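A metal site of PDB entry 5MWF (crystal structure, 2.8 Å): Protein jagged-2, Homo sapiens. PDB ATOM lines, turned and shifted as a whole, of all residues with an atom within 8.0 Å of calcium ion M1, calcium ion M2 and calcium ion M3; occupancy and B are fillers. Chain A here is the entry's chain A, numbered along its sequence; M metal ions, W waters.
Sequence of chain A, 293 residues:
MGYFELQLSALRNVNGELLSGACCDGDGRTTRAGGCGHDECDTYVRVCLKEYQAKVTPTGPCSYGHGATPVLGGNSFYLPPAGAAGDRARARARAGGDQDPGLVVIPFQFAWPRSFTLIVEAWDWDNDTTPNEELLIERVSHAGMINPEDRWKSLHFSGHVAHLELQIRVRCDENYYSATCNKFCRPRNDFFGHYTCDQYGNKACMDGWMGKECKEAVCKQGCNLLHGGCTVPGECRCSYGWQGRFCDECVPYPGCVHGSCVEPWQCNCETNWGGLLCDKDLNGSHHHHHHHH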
ATOM      1  N   LEU A  18      24.228   5.393  12.309  1.00  0.00           N
ATOM      2  CA  LEU A  18      23.001   4.711  11.943  1.00  0.00           C
ATOM      3  C   LEU A  18      22.671   5.084  10.512  1.00  0.00           C
ATOM      4  O   LEU A  18      23.322   5.930   9.906  1.00  0.00           O
ATOM      5  CB  LEU A  18      21.853   5.078  12.895  1.00  0.00           C
ATOM      6  CG  LEU A  18      22.099   4.864  14.392  1.00  0.00           C
ATOM      7  CD1 LEU A  18      21.158   5.722  15.221  1.00  0.00           C
ATOM      8  CD2 LEU A  18      21.958   3.408  14.763  1.00  0.00           C
ATOM      9  N   CYS A  23      25.002   9.242  15.410  1.00  0.00           N
ATOM     10  CA  CYS A  23      25.799   8.216  16.043  1.00  0.00           C
ATOM     11  C   CYS A  23      24.895   7.266  16.809  1.00  0.00           C
ATOM     12  O   CYS A  23      23.806   7.627  17.258  1.00  0.00           O
ATOM     13  CB  CYS A  23      26.840   8.843  16.987  1.00  0.00           C
ATOM     14  SG  CYS A  23      28.031   9.989  16.228  1.00  0.00           S
ATOM     15  N   CYS A  24      25.363   6.019  16.955  1.00  0.00           N
ATOM     16  CA  CYS A  24      24.536   4.974  17.555  1.00  0.00           C
ATOM     17  C   CYS A  24      24.133   5.338  18.983  1.00  0.00           C
ATOM     18  O   CYS A  24      22.937   5.372  19.313  1.00  0.00           O
ATOM     19  CB  CYS A  24      25.282   3.637  17.537  1.00  0.00           C
ATOM     20  SG  CYS A  24      25.283   2.770  15.963  1.00  0.00           S
ATOM     21  N   ASP A  25      25.120   5.617  19.828  1.00  0.00           N
ATOM     22  CA  ASP A  25      24.881   5.920  21.236  1.00  0.00           C
ATOM     23  C   ASP A  25      25.511   7.274  21.537  1.00  0.00           C
ATOM     24  O   ASP A  25      26.731   7.391  21.621  1.00  0.00           O
ATOM     25  CB  ASP A  25      25.451   4.828  22.142  1.00  0.00           C
ATOM     26  CG  ASP A  25      24.690   3.527  22.032  1.00  0.00           C
ATOM     27  OD1 ASP A  25      23.516   3.548  21.618  1.00  0.00           O
ATOM     28  OD2 ASP A  25      25.266   2.467  22.373  1.00  0.00           O
ATOM     29  N   GLY A  26      24.668   8.288  21.685  1.00  0.00           N
ATOM     30  CA  GLY A  26      25.149   9.607  22.000  1.00  0.00           C
ATOM     31  C   GLY A  26      24.562  10.695  21.132  1.00  0.00           C
ATOM     32  O   GLY A  26      24.470  10.550  19.910  1.00  0.00           O
ATOM     33  N   HIS A  38      33.535   6.697  22.117  1.00  0.00           N
ATOM     34  CA  HIS A  38      33.908   5.364  22.576  1.00  0.00           C
ATOM     35  C   HIS A  38      32.717   4.479  22.897  1.00  0.00           C
ATOM     36  O   HIS A  38      32.880   3.264  22.963  1.00  0.00           O
ATOM     37  CB  HIS A  38      34.790   5.443  23.826  1.00  0.00           C
ATOM     38  CG  HIS A  38      36.174   5.969  23.573  1.00  0.00           C
ATOM     39  ND1 HIS A  38      37.164   5.929  24.531  1.00  0.00           N
ATOM     40  CD2 HIS A  38      36.727   6.533  22.483  1.00  0.00           C
ATOM     41  CE1 HIS A  38      38.278   6.447  24.031  1.00  0.00           C
ATOM     42  NE2 HIS A  38      38.029   6.825  22.791  1.00  0.00           N
ATOM     43  N   ASP A  39      31.528   5.054  23.076  1.00  0.00           N
ATOM     44  CA  ASP A  39      30.319   4.232  23.171  1.00  0.00           C
ATOM     45  C   ASP A  39      29.938   3.832  21.749  1.00  0.00           C
ATOM     46  O   ASP A  39      29.349   4.616  21.009  1.00  0.00           O
ATOM     47  CB  ASP A  39      29.201   4.986  23.873  1.00  0.00           C
ATOM     48  CG  ASP A  39      28.103   4.060  24.362  1.00  0.00           C
ATOM     49  OD1 ASP A  39      27.962   2.955  23.798  1.00  0.00           O
ATOM     50  OD2 ASP A  39      27.376   4.441  25.306  1.00  0.00           O
ATOM     51  N   GLU A  40      30.278   2.603  21.373  1.00  0.00           N
ATOM     52  CA  GLU A  40      30.088   2.111  20.029  1.00  0.00           C
ATOM     53  C   GLU A  40      28.673   1.545  19.838  1.00  0.00           C
ATOM     54  O   GLU A  40      27.880   1.464  20.776  1.00  0.00           O
ATOM     55  CB  GLU A  40      31.129   1.034  19.686  1.00  0.00           C
ATOM     56  CG  GLU A  40      32.568   1.492  19.822  1.00  0.00           C
ATOM     57  CD  GLU A  40      33.560   0.420  19.418  1.00  0.00           C
ATOM     58  OE1 GLU A  40      34.552   0.750  18.726  1.00  0.00           O
ATOM     59  OE2 GLU A  40      33.359  -0.760  19.783  1.00  0.00           O
ATOM     60  N   CYS A  41      28.375   1.186  18.598  1.00  0.00           N
ATOM     61  CA  CYS A  41      27.113   0.513  18.290  1.00  0.00           C
ATOM     62  C   CYS A  41      27.084  -0.851  18.953  1.00  0.00           C
ATOM     63  O   CYS A  41      28.082  -1.580  18.970  1.00  0.00           O
ATOM     64  CB  CYS A  41      26.926   0.370  16.788  1.00  0.00           C
ATOM     65  SG  CYS A  41      27.118   1.902  15.872  1.00  0.00           S
ATOM     66  N   ASP A  42      25.939  -1.195  19.531  1.00  0.00           N
ATOM     67  CA  ASP A  42      25.710  -2.510  20.141  1.00  0.00           C
ATOM     68  C   ASP A  42      24.932  -3.337  19.114  1.00  0.00           C
ATOM     69  O   ASP A  42      23.700  -3.398  19.132  1.00  0.00           O
ATOM     70  CB  ASP A  42      24.957  -2.339  21.457  1.00  0.00           C
ATOM     71  CG  ASP A  42      25.627  -1.320  22.370  1.00  0.00           C
ATOM     72  OD1 ASP A  42      26.884  -1.326  22.435  1.00  0.00           O
ATOM     73  OD2 ASP A  42      24.931  -0.471  22.977  1.00  0.00           O
ATOM     74  N   THR A  43      25.667  -3.989  18.221  1.00  0.00           N
ATOM     75  CA  THR A  43      25.115  -4.475  16.961  1.00  0.00           C
ATOM     76  C   THR A  43      24.572  -5.889  17.081  1.00  0.00           C
ATOM     77  O   THR A  43      25.277  -6.793  17.532  1.00  0.00           O
ATOM     78  CB  THR A  43      26.174  -4.430  15.863  1.00  0.00           C
ATOM     79  OG1 THR A  43      26.684  -3.096  15.729  1.00  0.00           O
ATOM     80  CG2 THR A  43      25.578  -4.862  14.528  1.00  0.00           C
ATOM     81  N   VAL A  71      23.605  -9.268  20.802  1.00  0.00           N
ATOM     82  CA  VAL A  71      24.641  -8.335  20.403  1.00  0.00           C
ATOM     83  C   VAL A  71      25.913  -9.106  20.093  1.00  0.00           C
ATOM     84  O   VAL A  71      26.451  -9.820  20.954  1.00  0.00           O
ATOM     85  CB  VAL A  71      24.887  -7.283  21.498  1.00  0.00           C
ATOM     86  CG1 VAL A  71      26.091  -6.425  21.137  1.00  0.00           C
ATOM     87  CG2 VAL A  71      23.657  -6.410  21.667  1.00  0.00           C
ATOM     88  N   GLY A  73      28.812  -7.601  18.633  1.00  0.00           N
ATOM     89  CA  GLY A  73      30.022  -6.828  18.808  1.00  0.00           C
ATOM     90  C   GLY A  73      29.758  -5.333  18.753  1.00  0.00           C
ATOM     91  O   GLY A  73      28.643  -4.869  19.012  1.00  0.00           O
ATOM     92  N   GLY A  74      30.803  -4.588  18.416  1.00  0.00           N
ATOM     93  CA  GLY A  74      30.725  -3.145  18.369  1.00  0.00           C
ATOM     94  C   GLY A  74      30.479  -2.597  16.983  1.00  0.00           C
ATOM     95  O   GLY A  74      29.626  -3.093  16.256  1.00  0.00           O
ATOM     96  N   ASN A  75      31.249  -1.575  16.597  1.00  0.00           N
ATOM     97  CA  ASN A  75      31.072  -0.973  15.282  1.00  0.00           C
ATOM     98  C   ASN A  75      31.516  -1.917  14.173  1.00  0.00           C
ATOM     99  O   ASN A  75      30.878  -1.974  13.112  1.00  0.00           O
ATOM    100  CB  ASN A  75      31.836   0.337  15.192  1.00  0.00           C
ATOM    101  CG  ASN A  75      31.344   1.367  16.178  1.00  0.00           C
ATOM    102  OD1 ASN A  75      30.196   1.315  16.632  1.00  0.00           O
ATOM    103  ND2 ASN A  75      32.210   2.315  16.527  1.00  0.00           N
ATOM    104  N   TRP A 123      20.971  -3.718  13.730  1.00  0.00           N
ATOM    105  CA  TRP A 123      20.314  -2.826  14.667  1.00  0.00           C
ATOM    106  C   TRP A 123      21.219  -2.515  15.854  1.00  0.00           C
ATOM    107  O   TRP A 123      22.042  -3.337  16.259  1.00  0.00           O
ATOM    108  CB  TRP A 123      19.000  -3.435  15.191  1.00  0.00           C
ATOM    109  CG  TRP A 123      17.908  -3.575  14.176  1.00  0.00           C
ATOM    110  CD1 TRP A 123      17.744  -4.595  13.284  1.00  0.00           C
ATOM    111  CD2 TRP A 123      16.833  -2.668  13.947  1.00  0.00           C
ATOM    112  NE1 TRP A 123      16.617  -4.382  12.515  1.00  0.00           N
ATOM    113  CE2 TRP A 123      16.044  -3.200  12.914  1.00  0.00           C
ATOM    114  CE3 TRP A 123      16.454  -1.448  14.528  1.00  0.00           C
ATOM    115  CZ2 TRP A 123      14.903  -2.554  12.434  1.00  0.00           C
ATOM    116  CZ3 TRP A 123      15.317  -0.818  14.056  1.00  0.00           C
ATOM    117  CH2 TRP A 123      14.559  -1.370  13.020  1.00  0.00           C
ATOM    118  N   ASP A 124      21.041  -1.309  16.406  1.00  0.00           N
ATOM    119  CA  ASP A 124      21.675  -0.921  17.659  1.00  0.00           C
ATOM    120  C   ASP A 124      20.766  -1.269  18.824  1.00  0.00           C
ATOM    121  O   ASP A 124      19.544  -1.082  18.767  1.00  0.00           O
ATOM    122  CB  ASP A 124      21.989   0.586  17.670  1.00  0.00           C
ATOM    123  CG  ASP A 124      22.563   1.063  18.999  1.00  0.00           C
ATOM    124  OD1 ASP A 124      23.310   0.310  19.655  1.00  0.00           O
ATOM    125  OD2 ASP A 124      22.262   2.215  19.401  1.00  0.00           O
ATOM    126  N   TRP A 125      21.377  -1.779  19.893  1.00  0.00           N
ATOM    127  CA  TRP A 125      20.666  -2.259  21.075  1.00  0.00           C
ATOM    128  C   TRP A 125      20.858  -1.267  22.213  1.00  0.00           C
ATOM    129  O   TRP A 125      22.001  -0.884  22.520  1.00  0.00           O
ATOM    130  CB  TRP A 125      21.159  -3.653  21.466  1.00  0.00           C
ATOM    131  CG  TRP A 125      20.503  -4.250  22.667  1.00  0.00           C
ATOM    132  CD1 TRP A 125      21.072  -4.514  23.873  1.00  0.00           C
ATOM    133  CD2 TRP A 125      19.138  -4.665  22.783  1.00  0.00           C
ATOM    134  NE1 TRP A 125      20.170  -5.058  24.732  1.00  0.00           N
ATOM    135  CE2 TRP A 125      18.960  -5.167  24.089  1.00  0.00           C
ATOM    136  CE3 TRP A 125      18.037  -4.657  21.908  1.00  0.00           C
ATOM    137  CZ2 TRP A 125      17.738  -5.653  24.545  1.00  0.00           C
ATOM    138  CZ3 TRP A 125      16.825  -5.144  22.367  1.00  0.00           C
ATOM    139  CH2 TRP A 125      16.687  -5.634  23.665  1.00  0.00           C
ATOM    140  N   ASP A 126      19.749  -0.857  22.828  1.00  0.00           N
ATOM    141  CA  ASP A 126      19.782   0.021  23.989  1.00  0.00           C
ATOM    142  C   ASP A 126      18.996  -0.571  25.158  1.00  0.00           C
ATOM    143  O   ASP A 126      18.388   0.169  25.939  1.00  0.00           O
ATOM    144  CB  ASP A 126      19.259   1.427  23.648  1.00  0.00           C
ATOM    145  CG  ASP A 126      19.969   2.049  22.462  1.00  0.00           C
ATOM    146  OD1 ASP A 126      21.193   1.834  22.303  1.00  0.00           O
ATOM    147  OD2 ASP A 126      19.316   2.801  21.699  1.00  0.00           O
ATOM    148  N   ASN A 127      19.014  -1.898  25.293  1.00  0.00           N
ATOM    149  CA  ASN A 127      18.396  -2.594  26.414  1.00  0.00           C
ATOM    150  C   ASN A 127      16.935  -2.195  26.591  1.00  0.00           C
ATOM    151  O   ASN A 127      16.460  -1.946  27.704  1.00  0.00           O
ATOM    152  CB  ASN A 127      19.192  -2.375  27.699  1.00  0.00           C
ATOM    153  CG  ASN A 127      20.572  -3.005  27.638  1.00  0.00           C
ATOM    154  OD1 ASN A 127      21.529  -2.357  27.226  1.00  0.00           O
ATOM    155  ND2 ASN A 127      20.665  -4.270  28.032  1.00  0.00           N
ATOM    156  N   ASN A 132      11.806   0.704  17.673  1.00  0.00           N
ATOM    157  CA  ASN A 132      12.271   2.064  17.404  1.00  0.00           C
ATOM    158  C   ASN A 132      13.018   2.050  16.077  1.00  0.00           C
ATOM    159  O   ASN A 132      14.204   1.690  16.032  1.00  0.00           O
ATOM    160  CB  ASN A 132      13.144   2.573  18.535  1.00  0.00           C
ATOM    161  CG  ASN A 132      13.497   4.054  18.399  1.00  0.00           C
ATOM    162  OD1 ASN A 132      13.316   4.650  17.334  1.00  0.00           O
ATOM    163  ND2 ASN A 132      14.023   4.633  19.465  1.00  0.00           N
ATOM    164  N   GLU A 134      14.400   4.154  14.373  1.00  0.00           N
ATOM    165  CA  GLU A 134      15.548   5.045  14.248  1.00  0.00           C
ATOM    166  C   GLU A 134      16.842   4.410  14.718  1.00  0.00           C
ATOM    167  O   GLU A 134      17.891   5.054  14.645  1.00  0.00           O
ATOM    168  CB  GLU A 134      15.280   6.345  15.018  1.00  0.00           C
ATOM    169  CG  GLU A 134      14.019   7.041  14.554  1.00  0.00           C
ATOM    170  CD  GLU A 134      14.122   8.537  14.603  1.00  0.00           C
ATOM    171  OE1 GLU A 134      13.350   9.158  15.367  1.00  0.00           O
ATOM    172  OE2 GLU A 134      14.986   9.089  13.883  1.00  0.00           O
ATOM    173  N   LEU A 135      16.793   3.171  15.215  1.00  0.00           N
ATOM    174  CA  LEU A 135      17.986   2.438  15.615  1.00  0.00           C
ATOM    175  C   LEU A 135      18.507   1.518  14.520  1.00  0.00           C
ATOM    176  O   LEU A 135      19.333   0.642  14.795  1.00  0.00           O
ATOM    177  CB  LEU A 135      17.711   1.645  16.895  1.00  0.00           C
ATOM    178  CG  LEU A 135      17.083   2.431  18.059  1.00  0.00           C
ATOM    179  CD1 LEU A 135      16.525   1.467  19.092  1.00  0.00           C
ATOM    180  CD2 LEU A 135      18.103   3.368  18.681  1.00  0.00           C
HETATM  181 CA    CA M   1      23.236   1.125  22.027  1.00  0.00          CA
HETATM  182 CA    CA M   2      27.011   1.020  22.940  1.00  0.00          CA
HETATM  183 CA    CA M   3      21.284   3.925  20.943  1.00  0.00          CA
HETATM  184  O   HOH W   1      21.191   6.956  22.308  1.00  0.00           O
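The side-chain amide nitrogen of Asn 127 lies close to the indole nitrogen of Trp 125 (3.4 Å).
N of Asp 124 sits at hydrogen-bond distance from O of Leu 135 (3.1 Å).
The side-chain sulfur (SG) of Cys 24 forms a disulfide with the side-chain sulfur (SG) of Cys 41, at 2.0 Å.
Along chain A the residues within 4 Å of calcium ion M2 span positions 25 to 42.
Leu 135 touches calcium ion M3 (CD2 to CA, 3.9 Å).
Within 4 Å of calcium ion M3: Cys 24, Asp 25, Asp 124, Asp 126 and Leu 135.
The nearest printed residue that does not touch calcium ion M3 is Trp 125 (5.1 Å).
Calcium ion M1 is bound by OD1 of Asp 126, O of Trp 125, OD2 of Asp 25, OD1 of Asp 25, OD1 of Asp 124 and OD2 of Asp 42.
Slightly farther from calcium ion M1 lies OD2 of Asp 124 (3.0 Å).
Calcium ion M3 is bound by the side-chain carboxylate (OD1) of Asp 25 (2.4 Å), the side-chain carboxylate (OD2) of Asp 126 (2.4 Å), the side-chain carboxylate (OD1) of Asp 126 (2.5 Å), the side-chain carboxylate (OD2) of Asp 124 (2.5 Å) and the backbone carbonyl oxygen (O) of Cys 24 (2.7 Å).
Calcium ion M3 has five donor atoms within binding distance.
Calcium ion M2 is bound by OD1 of Asp 39 (2.3 Å), OD2 of Asp 25 (2.3 Å), O of Glu 40 (2.4 Å), OD1 of Asp 42 (2.4 Å) and OD2 of Asp 42 (2.6 Å).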
